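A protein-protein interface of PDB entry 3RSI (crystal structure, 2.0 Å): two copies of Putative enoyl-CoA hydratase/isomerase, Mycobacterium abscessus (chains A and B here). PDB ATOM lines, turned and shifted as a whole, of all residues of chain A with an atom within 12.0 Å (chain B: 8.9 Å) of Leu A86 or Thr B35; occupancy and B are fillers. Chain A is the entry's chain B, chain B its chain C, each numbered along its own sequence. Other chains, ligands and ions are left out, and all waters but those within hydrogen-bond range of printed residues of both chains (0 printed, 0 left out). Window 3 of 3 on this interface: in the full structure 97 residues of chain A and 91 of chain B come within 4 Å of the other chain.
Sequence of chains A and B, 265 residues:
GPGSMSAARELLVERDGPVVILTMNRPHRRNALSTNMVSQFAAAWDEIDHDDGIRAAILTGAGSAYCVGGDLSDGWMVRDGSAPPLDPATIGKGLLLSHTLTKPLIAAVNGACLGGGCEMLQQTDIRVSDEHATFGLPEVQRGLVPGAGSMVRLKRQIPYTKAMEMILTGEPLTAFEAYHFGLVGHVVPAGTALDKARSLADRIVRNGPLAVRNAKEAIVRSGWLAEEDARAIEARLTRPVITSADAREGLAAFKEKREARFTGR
Leu A86 touches Thr B35. CB of Ala B42 touches O of Thr A90, at 3.7 Å. CG of Lys A93 touches CB of Ala B42, at 3.9 Å. Val B38 touches Gly A94 (O to CA, 3.5 Å). Phe B41 touches Gly A94 (CB to O, 3.5 Å). Ala B42 touches Gly A94. Leu B33 touches Leu A95 (CD1 to CD2, 3.8 Å). Leu A95 touches Val B38. CA of Gly A116 touches CD1 of Leu B33, 3.8 Å away. Phe B41 touches Met A120.
Leu A86 touches just these residues of chain B: Thr B35 and Ser B39. Thr B35 touches one residue of chain A. No residue of chain A comes within 4 Å of Ser B34. Of chain A, only Ile A91 (3.9 Å), Gly A94 (3.5 Å) and Leu A95 (3.8 Å) come within 4 Å of Val B38. Ser B39 touches just one residue of chain A: Leu A86. Printed residues of chain B within 4 Å of Met A120: Phe B41 (3.8 Å). Of the printed residues of chain A, Leu B33 touches Leu A95 (3.8 Å) and Gly A116 (3.8 Å). The nearest residue of chain A that does not touch Thr B35 is Thr A90 (6.5 Å).
Hydrophobic or aromatic side chains of chain A within 4 Å of the printed part of chain B: Leu A86, Leu A95 and Met A120. Of the 14 printed residues of chain B, 6 touch a printed residue of chain A. Printed residues of chain B that touch a printed residue of chain A: Leu B33, Thr B35, Val B38, Ser B39, Phe B41 and Ala B42. Hydrophobic or aromatic side chains of chain B that line the printed part of chain A: Leu B33, Val B38, Phe B41 and Ala B42. Among the printed residues, 12 pairs touch across the chains.
No position is printed for both chains. Of the 12 pairs that touch across the chains among the printed residues, none has its exchanged pair printed and touching as well.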
ATOM      1  N   LEU A  86       4.882  -2.961 -17.749  1.00  0.00           N
ATOM      2  CA  LEU A  86       4.321  -2.864 -19.085  1.00  0.00           C
ATOM      3  C   LEU A  86       2.902  -2.287 -19.074  1.00  0.00           C
ATOM      4  O   LEU A  86       2.208  -2.334 -18.060  1.00  0.00           O
ATOM      5  CB  LEU A  86       4.283  -4.251 -19.744  1.00  0.00           C
ATOM      6  CG  LEU A  86       5.593  -4.825 -20.297  1.00  0.00           C
ATOM      7  CD1 LEU A  86       5.427  -6.313 -20.640  1.00  0.00           C
ATOM      8  CD2 LEU A  86       6.064  -4.016 -21.514  1.00  0.00           C
ATOM      9  N   ASP A  87       2.516  -1.738 -20.224  1.00  0.00           N
ATOM     10  CA  ASP A  87       1.135  -1.409 -20.584  1.00  0.00           C
ATOM     11  C   ASP A  87       0.194  -2.631 -20.358  1.00  0.00           C
ATOM     12  O   ASP A  87       0.536  -3.743 -20.755  1.00  0.00           O
ATOM     13  CB  ASP A  87       1.166  -1.053 -22.084  1.00  0.00           C
ATOM     14  CG  ASP A  87      -0.115  -0.412 -22.592  1.00  0.00           C
ATOM     15  OD1 ASP A  87      -1.220  -0.668 -22.047  1.00  0.00           O
ATOM     16  OD2 ASP A  87      -0.006   0.350 -23.592  1.00  0.00           O
ATOM     17  N   PRO A  88      -0.993  -2.432 -19.738  1.00  0.00           N
ATOM     18  CA  PRO A  88      -1.951  -3.544 -19.604  1.00  0.00           C
ATOM     19  C   PRO A  88      -2.408  -4.167 -20.929  1.00  0.00           C
ATOM     20  O   PRO A  88      -2.673  -5.353 -20.978  1.00  0.00           O
ATOM     21  CB  PRO A  88      -3.146  -2.920 -18.882  1.00  0.00           C
ATOM     22  CG  PRO A  88      -2.851  -1.486 -18.727  1.00  0.00           C
ATOM     23  CD  PRO A  88      -1.416  -1.246 -18.972  1.00  0.00           C
ATOM     24  N   ALA A  89      -2.524  -3.355 -21.975  1.00  0.00           N
ATOM     25  CA  ALA A  89      -2.755  -3.850 -23.335  1.00  0.00           C
ATOM     26  C   ALA A  89      -1.640  -4.810 -23.773  1.00  0.00           C
ATOM     27  O   ALA A  89      -1.903  -5.889 -24.305  1.00  0.00           O
ATOM     28  CB  ALA A  89      -2.869  -2.673 -24.324  1.00  0.00           C
ATOM     29  N   THR A  90      -0.393  -4.414 -23.538  1.00  0.00           N
ATOM     30  CA  THR A  90       0.747  -5.230 -23.949  1.00  0.00           C
ATOM     31  C   THR A  90       0.778  -6.531 -23.159  1.00  0.00           C
ATOM     32  O   THR A  90       0.901  -7.613 -23.742  1.00  0.00           O
ATOM     33  CB  THR A  90       2.082  -4.464 -23.774  1.00  0.00           C
ATOM     34  OG1 THR A  90       2.029  -3.277 -24.568  1.00  0.00           O
ATOM     35  CG2 THR A  90       3.238  -5.319 -24.239  1.00  0.00           C
ATOM     36  N   ILE A  91       0.621  -6.432 -21.837  1.00  0.00           N
ATOM     37  CA  ILE A  91       0.626  -7.631 -20.984  1.00  0.00           C
ATOM     38  C   ILE A  91      -0.488  -8.609 -21.386  1.00  0.00           C
ATOM     39  O   ILE A  91      -0.239  -9.805 -21.585  1.00  0.00           O
ATOM     40  CB  ILE A  91       0.450  -7.298 -19.506  1.00  0.00           C
ATOM     41  CG1 ILE A  91       1.624  -6.451 -18.993  1.00  0.00           C
ATOM     42  CG2 ILE A  91       0.359  -8.597 -18.694  1.00  0.00           C
ATOM     43  CD1 ILE A  91       1.383  -5.839 -17.590  1.00  0.00           C
ATOM     44  N   GLY A  92      -1.715  -8.100 -21.496  1.00  0.00           N
ATOM     45  CA  GLY A  92      -2.872  -8.938 -21.835  1.00  0.00           C
ATOM     46  C   GLY A  92      -2.708  -9.635 -23.167  1.00  0.00           C
ATOM     47  O   GLY A  92      -2.983 -10.847 -23.285  1.00  0.00           O
ATOM     48  N   LYS A  93      -2.232  -8.878 -24.156  1.00  0.00           N
ATOM     49  CA  LYS A  93      -1.950  -9.411 -25.479  1.00  0.00           C
ATOM     50  C   LYS A  93      -0.805 -10.429 -25.469  1.00  0.00           C
ATOM     51  O   LYS A  93      -0.938 -11.469 -26.066  1.00  0.00           O
ATOM     52  CB  LYS A  93      -1.631  -8.281 -26.473  1.00  0.00           C
ATOM     53  CG  LYS A  93      -1.113  -8.750 -27.810  1.00  0.00           C
ATOM     54  CD  LYS A  93      -1.076  -7.620 -28.827  1.00  0.00           C
ATOM     55  CE  LYS A  93      -2.463  -7.378 -29.441  1.00  0.00           C
ATOM     56  NZ  LYS A  93      -2.479  -6.121 -30.219  1.00  0.00           N
ATOM     57  N   GLY A  94       0.319 -10.111 -24.834  1.00  0.00           N
ATOM     58  CA  GLY A  94       1.466 -11.021 -24.809  1.00  0.00           C
ATOM     59  C   GLY A  94       1.149 -12.401 -24.232  1.00  0.00           C
ATOM     60  O   GLY A  94       1.557 -13.436 -24.779  1.00  0.00           O
ATOM     61  N   LEU A  95       0.420 -12.394 -23.117  1.00  0.00           N
ATOM     62  CA  LEU A  95      -0.029 -13.606 -22.436  1.00  0.00           C
ATOM     63  C   LEU A  95      -1.180 -14.309 -23.125  1.00  0.00           C
ATOM     64  O   LEU A  95      -1.631 -15.360 -22.652  1.00  0.00           O
ATOM     65  CB  LEU A  95      -0.461 -13.277 -20.992  1.00  0.00           C
ATOM     66  CG  LEU A  95       0.620 -12.753 -20.042  1.00  0.00           C
ATOM     67  CD1 LEU A  95       0.046 -12.470 -18.654  1.00  0.00           C
ATOM     68  CD2 LEU A  95       1.765 -13.751 -19.936  1.00  0.00           C
ATOM     69  N   LEU A  96      -1.660 -13.747 -24.237  1.00  0.00           N
ATOM     70  CA  LEU A  96      -2.904 -14.205 -24.889  1.00  0.00           C
ATOM     71  C   LEU A  96      -4.073 -14.316 -23.896  1.00  0.00           C
ATOM     72  O   LEU A  96      -4.940 -15.219 -23.997  1.00  0.00           O
ATOM     73  CB  LEU A  96      -2.658 -15.538 -25.611  1.00  0.00           C
ATOM     74  CG  LEU A  96      -1.671 -15.453 -26.782  1.00  0.00           C
ATOM     75  CD1 LEU A  96      -1.484 -16.813 -27.402  1.00  0.00           C
ATOM     76  CD2 LEU A  96      -2.146 -14.429 -27.829  1.00  0.00           C
ATOM     77  N   LEU A  97      -4.087 -13.403 -22.927  1.00  0.00           N
ATOM     78  CA  LEU A  97      -5.142 -13.349 -21.947  1.00  0.00           C
ATOM     79  C   LEU A  97      -6.326 -12.546 -22.512  1.00  0.00           C
ATOM     80  O   LEU A  97      -7.465 -12.983 -22.470  1.00  0.00           O
ATOM     81  CB  LEU A  97      -4.618 -12.722 -20.663  1.00  0.00           C
ATOM     82  CG  LEU A  97      -5.520 -12.799 -19.432  1.00  0.00           C
ATOM     83  CD1 LEU A  97      -6.124 -14.182 -19.310  1.00  0.00           C
ATOM     84  CD2 LEU A  97      -4.736 -12.408 -18.161  1.00  0.00           C
ATOM     85  N   SER A  98      -6.045 -11.361 -23.023  1.00  0.00           N
ATOM     86  CA  SER A  98      -7.064 -10.546 -23.669  1.00  0.00           C
ATOM     87  C   SER A  98      -6.975 -10.589 -25.184  1.00  0.00           C
ATOM     88  O   SER A  98      -7.687  -9.861 -25.857  1.00  0.00           O
ATOM     89  CB  SER A  98      -6.931  -9.095 -23.215  1.00  0.00           C
ATOM     90  OG  SER A  98      -5.706  -8.541 -23.669  1.00  0.00           O
ATOM     91  N   GLY A 116       2.936 -19.945 -15.830  1.00  0.00           N
ATOM     92  CA  GLY A 116       2.626 -19.099 -16.985  1.00  0.00           C
ATOM     93  C   GLY A 116       2.694 -19.817 -18.315  1.00  0.00           C
ATOM     94  O   GLY A 116       1.915 -19.540 -19.206  1.00  0.00           O
ATOM     95  N   MET A 120      -0.531 -20.044 -20.807  1.00  0.00           N
ATOM     96  CA  MET A 120      -0.537 -19.684 -22.225  1.00  0.00           C
ATOM     97  C   MET A 120      -0.869 -20.861 -23.172  1.00  0.00           C
ATOM     98  O   MET A 120      -1.414 -20.663 -24.270  1.00  0.00           O
ATOM     99  CB  MET A 120       0.788 -19.041 -22.634  1.00  0.00           C
ATOM    100  CG  MET A 120       0.915 -17.598 -22.197  1.00  0.00           C
ATOM    101  SD  MET A 120       2.506 -16.842 -22.643  1.00  0.00           S
ATOM    102  CE  MET A 120       2.288 -16.651 -24.411  1.00  0.00           C
ATOM    103  N   GLU B  10      15.219 -12.956 -25.941  1.00  0.00           N
ATOM    104  CA  GLU B  10      14.448 -13.761 -24.968  1.00  0.00           C
ATOM    105  C   GLU B  10      13.305 -14.543 -25.631  1.00  0.00           C
ATOM    106  O   GLU B  10      12.912 -15.599 -25.159  1.00  0.00           O
ATOM    107  CB  GLU B  10      13.968 -12.898 -23.785  1.00  0.00           C
ATOM    108  CG  GLU B  10      15.137 -12.466 -22.867  1.00  0.00           C
ATOM    109  CD  GLU B  10      14.734 -11.508 -21.754  1.00  0.00           C
ATOM    110  OE1 GLU B  10      13.802 -11.841 -21.004  1.00  0.00           O
ATOM    111  OE2 GLU B  10      15.365 -10.426 -21.611  1.00  0.00           O
ATOM    112  N   ARG B  26      15.245 -18.456 -22.602  1.00  0.00           N
ATOM    113  CA  ARG B  26      16.064 -18.172 -21.421  1.00  0.00           C
ATOM    114  C   ARG B  26      16.357 -19.489 -20.725  1.00  0.00           C
ATOM    115  O   ARG B  26      15.907 -19.705 -19.617  1.00  0.00           O
ATOM    116  CB  ARG B  26      15.330 -17.237 -20.473  1.00  0.00           C
ATOM    117  CG  ARG B  26      14.867 -15.951 -21.115  1.00  0.00           C
ATOM    118  CD  ARG B  26      13.950 -15.238 -20.189  1.00  0.00           C
ATOM    119  NE  ARG B  26      14.694 -14.663 -19.075  1.00  0.00           N
ATOM    120  CZ  ARG B  26      14.284 -14.626 -17.812  1.00  0.00           C
ATOM    121  NH1 ARG B  26      13.121 -15.164 -17.440  1.00  0.00           N
ATOM    122  NH2 ARG B  26      15.065 -14.040 -16.915  1.00  0.00           N
ATOM    123  N   ARG B  29      16.999 -20.145 -17.098  1.00  0.00           N
ATOM    124  CA  ARG B  29      15.838 -20.046 -16.202  1.00  0.00           C
ATOM    125  C   ARG B  29      14.670 -20.946 -16.647  1.00  0.00           C
ATOM    126  O   ARG B  29      13.508 -20.725 -16.276  1.00  0.00           O
ATOM    127  CB  ARG B  29      15.372 -18.591 -16.086  1.00  0.00           C
ATOM    128  CG  ARG B  29      16.339 -17.701 -15.313  1.00  0.00           C
ATOM    129  CD  ARG B  29      15.615 -16.545 -14.665  1.00  0.00           C
ATOM    130  NE  ARG B  29      14.654 -16.983 -13.645  1.00  0.00           N
ATOM    131  CZ  ARG B  29      13.510 -16.351 -13.344  1.00  0.00           C
ATOM    132  NH1 ARG B  29      13.148 -15.234 -13.974  1.00  0.00           N
ATOM    133  NH2 ARG B  29      12.711 -16.849 -12.403  1.00  0.00           N
ATOM    134  N   ALA B  32      11.446 -19.245 -18.249  1.00  0.00           N
ATOM    135  CA  ALA B  32      10.485 -18.509 -17.440  1.00  0.00           C
ATOM    136  C   ALA B  32      10.117 -17.200 -18.138  1.00  0.00           C
ATOM    137  O   ALA B  32      10.987 -16.537 -18.709  1.00  0.00           O
ATOM    138  CB  ALA B  32      11.083 -18.223 -16.047  1.00  0.00           C
ATOM    139  N   LEU B  33       8.827 -16.871 -18.128  1.00  0.00           N
ATOM    140  CA  LEU B  33       8.323 -15.607 -18.667  1.00  0.00           C
ATOM    141  C   LEU B  33       8.972 -14.462 -17.919  1.00  0.00           C
ATOM    142  O   LEU B  33       9.153 -14.522 -16.711  1.00  0.00           O
ATOM    143  CB  LEU B  33       6.791 -15.487 -18.528  1.00  0.00           C
ATOM    144  CG  LEU B  33       5.895 -16.514 -19.217  1.00  0.00           C
ATOM    145  CD1 LEU B  33       4.429 -16.304 -18.867  1.00  0.00           C
ATOM    146  CD2 LEU B  33       6.096 -16.453 -20.728  1.00  0.00           C
ATOM    147  N   SER B  34       9.356 -13.439 -18.662  1.00  0.00           N
ATOM    148  CA  SER B  34       9.865 -12.194 -18.103  1.00  0.00           C
ATOM    149  C   SER B  34       9.056 -11.057 -18.735  1.00  0.00           C
ATOM    150  O   SER B  34       8.299 -11.274 -19.673  1.00  0.00           O
ATOM    151  CB  SER B  34      11.354 -12.038 -18.412  1.00  0.00           C
ATOM    152  OG  SER B  34      11.620 -12.035 -19.809  1.00  0.00           O
ATOM    153  N   THR B  35       9.180  -9.861 -18.178  1.00  0.00           N
ATOM    154  CA  THR B  35       8.611  -8.647 -18.757  1.00  0.00           C
ATOM    155  C   THR B  35       8.967  -8.501 -20.232  1.00  0.00           C
ATOM    156  O   THR B  35       8.116  -8.249 -21.083  1.00  0.00           O
ATOM    157  CB  THR B  35       9.189  -7.404 -18.027  1.00  0.00           C
ATOM    158  OG1 THR B  35       8.994  -7.556 -16.619  1.00  0.00           O
ATOM    159  CG2 THR B  35       8.522  -6.135 -18.509  1.00  0.00           C
ATOM    160  N   ASN B  36      10.252  -8.637 -20.512  1.00  0.00           N
ATOM    161  CA  ASN B  36      10.752  -8.511 -21.853  1.00  0.00           C
ATOM    162  C   ASN B  36      10.140  -9.553 -22.809  1.00  0.00           C
ATOM    163  O   ASN B  36       9.772  -9.224 -23.950  1.00  0.00           O
ATOM    164  CB  ASN B  36      12.262  -8.642 -21.825  1.00  0.00           C
ATOM    165  CG  ASN B  36      12.886  -8.360 -23.153  1.00  0.00           C
ATOM    166  OD1 ASN B  36      13.408  -9.267 -23.811  1.00  0.00           O
ATOM    167  ND2 ASN B  36      12.828  -7.101 -23.578  1.00  0.00           N
ATOM    168  N   MET B  37      10.013 -10.792 -22.340  1.00  0.00           N
ATOM    169  CA  MET B  37       9.492 -11.864 -23.190  1.00  0.00           C
ATOM    170  C   MET B  37       8.022 -11.623 -23.515  1.00  0.00           C
ATOM    171  O   MET B  37       7.594 -11.825 -24.654  1.00  0.00           O
ATOM    172  CB  MET B  37       9.673 -13.238 -22.551  1.00  0.00           C
ATOM    173  CG  MET B  37       9.563 -14.353 -23.576  1.00  0.00           C
ATOM    174  SD  MET B  37       9.510 -16.001 -22.850  1.00  0.00           S
ATOM    175  CE  MET B  37      11.152 -16.159 -22.165  1.00  0.00           C
ATOM    176  N   VAL B  38       7.253 -11.210 -22.511  1.00  0.00           N
ATOM    177  CA  VAL B  38       5.832 -10.899 -22.722  1.00  0.00           C
ATOM    178  C   VAL B  38       5.668  -9.762 -23.725  1.00  0.00           C
ATOM    179  O   VAL B  38       4.793  -9.818 -24.613  1.00  0.00           O
ATOM    180  CB  VAL B  38       5.140 -10.551 -21.407  1.00  0.00           C
ATOM    181  CG1 VAL B  38       3.770  -9.878 -21.666  1.00  0.00           C
ATOM    182  CG2 VAL B  38       5.014 -11.815 -20.557  1.00  0.00           C
ATOM    183  N   SER B  39       6.520  -8.744 -23.590  1.00  0.00           N
ATOM    184  CA  SER B  39       6.532  -7.643 -24.531  1.00  0.00           C
ATOM    185  C   SER B  39       6.817  -8.141 -25.944  1.00  0.00           C
ATOM    186  O   SER B  39       6.130  -7.754 -26.897  1.00  0.00           O
ATOM    187  CB  SER B  39       7.585  -6.621 -24.131  1.00  0.00           C
ATOM    188  OG  SER B  39       7.512  -5.504 -24.971  1.00  0.00           O
ATOM    189  N   GLN B  40       7.829  -8.991 -26.080  1.00  0.00           N
ATOM    190  CA  GLN B  40       8.179  -9.548 -27.385  1.00  0.00           C
ATOM    191  C   GLN B  40       7.078 -10.469 -27.936  1.00  0.00           C
ATOM    192  O   GLN B  40       6.837 -10.502 -29.142  1.00  0.00           O
ATOM    193  CB  GLN B  40       9.517 -10.259 -27.308  1.00  0.00           C
ATOM    194  CG  GLN B  40      10.675  -9.266 -27.142  1.00  0.00           C
ATOM    195  CD  GLN B  40      12.011  -9.924 -26.847  1.00  0.00           C
ATOM    196  OE1 GLN B  40      12.126 -11.153 -26.816  1.00  0.00           O
ATOM    197  NE2 GLN B  40      13.039  -9.101 -26.630  1.00  0.00           N
ATOM    198  N   PHE B  41       6.424 -11.204 -27.038  1.00  0.00           N
ATOM    199  CA  PHE B  41       5.263 -12.008 -27.395  1.00  0.00           C
ATOM    200  C   PHE B  41       4.200 -11.126 -28.070  1.00  0.00           C
ATOM    201  O   PHE B  41       3.760 -11.429 -29.179  1.00  0.00           O
ATOM    202  CB  PHE B  41       4.685 -12.701 -26.161  1.00  0.00           C
ATOM    203  CG  PHE B  41       5.144 -14.125 -25.970  1.00  0.00           C
ATOM    204  CD1 PHE B  41       4.994 -15.066 -26.980  1.00  0.00           C
ATOM    205  CD2 PHE B  41       5.626 -14.544 -24.740  1.00  0.00           C
ATOM    206  CE1 PHE B  41       5.384 -16.393 -26.775  1.00  0.00           C
ATOM    207  CE2 PHE B  41       6.002 -15.866 -24.523  1.00  0.00           C
ATOM    208  CZ  PHE B  41       5.878 -16.792 -25.523  1.00  0.00           C
ATOM    209  N   ALA B  42       3.850 -10.008 -27.430  1.00  0.00           N
ATOM    210  CA  ALA B  42       2.830  -9.098 -27.984  1.00  0.00           C
ATOM    211  C   ALA B  42       3.203  -8.611 -29.386  1.00  0.00           C
ATOM    212  O   ALA B  42       2.380  -8.638 -30.296  1.00  0.00           O
ATOM    213  CB  ALA B  42       2.572  -7.925 -27.032  1.00  0.00           C
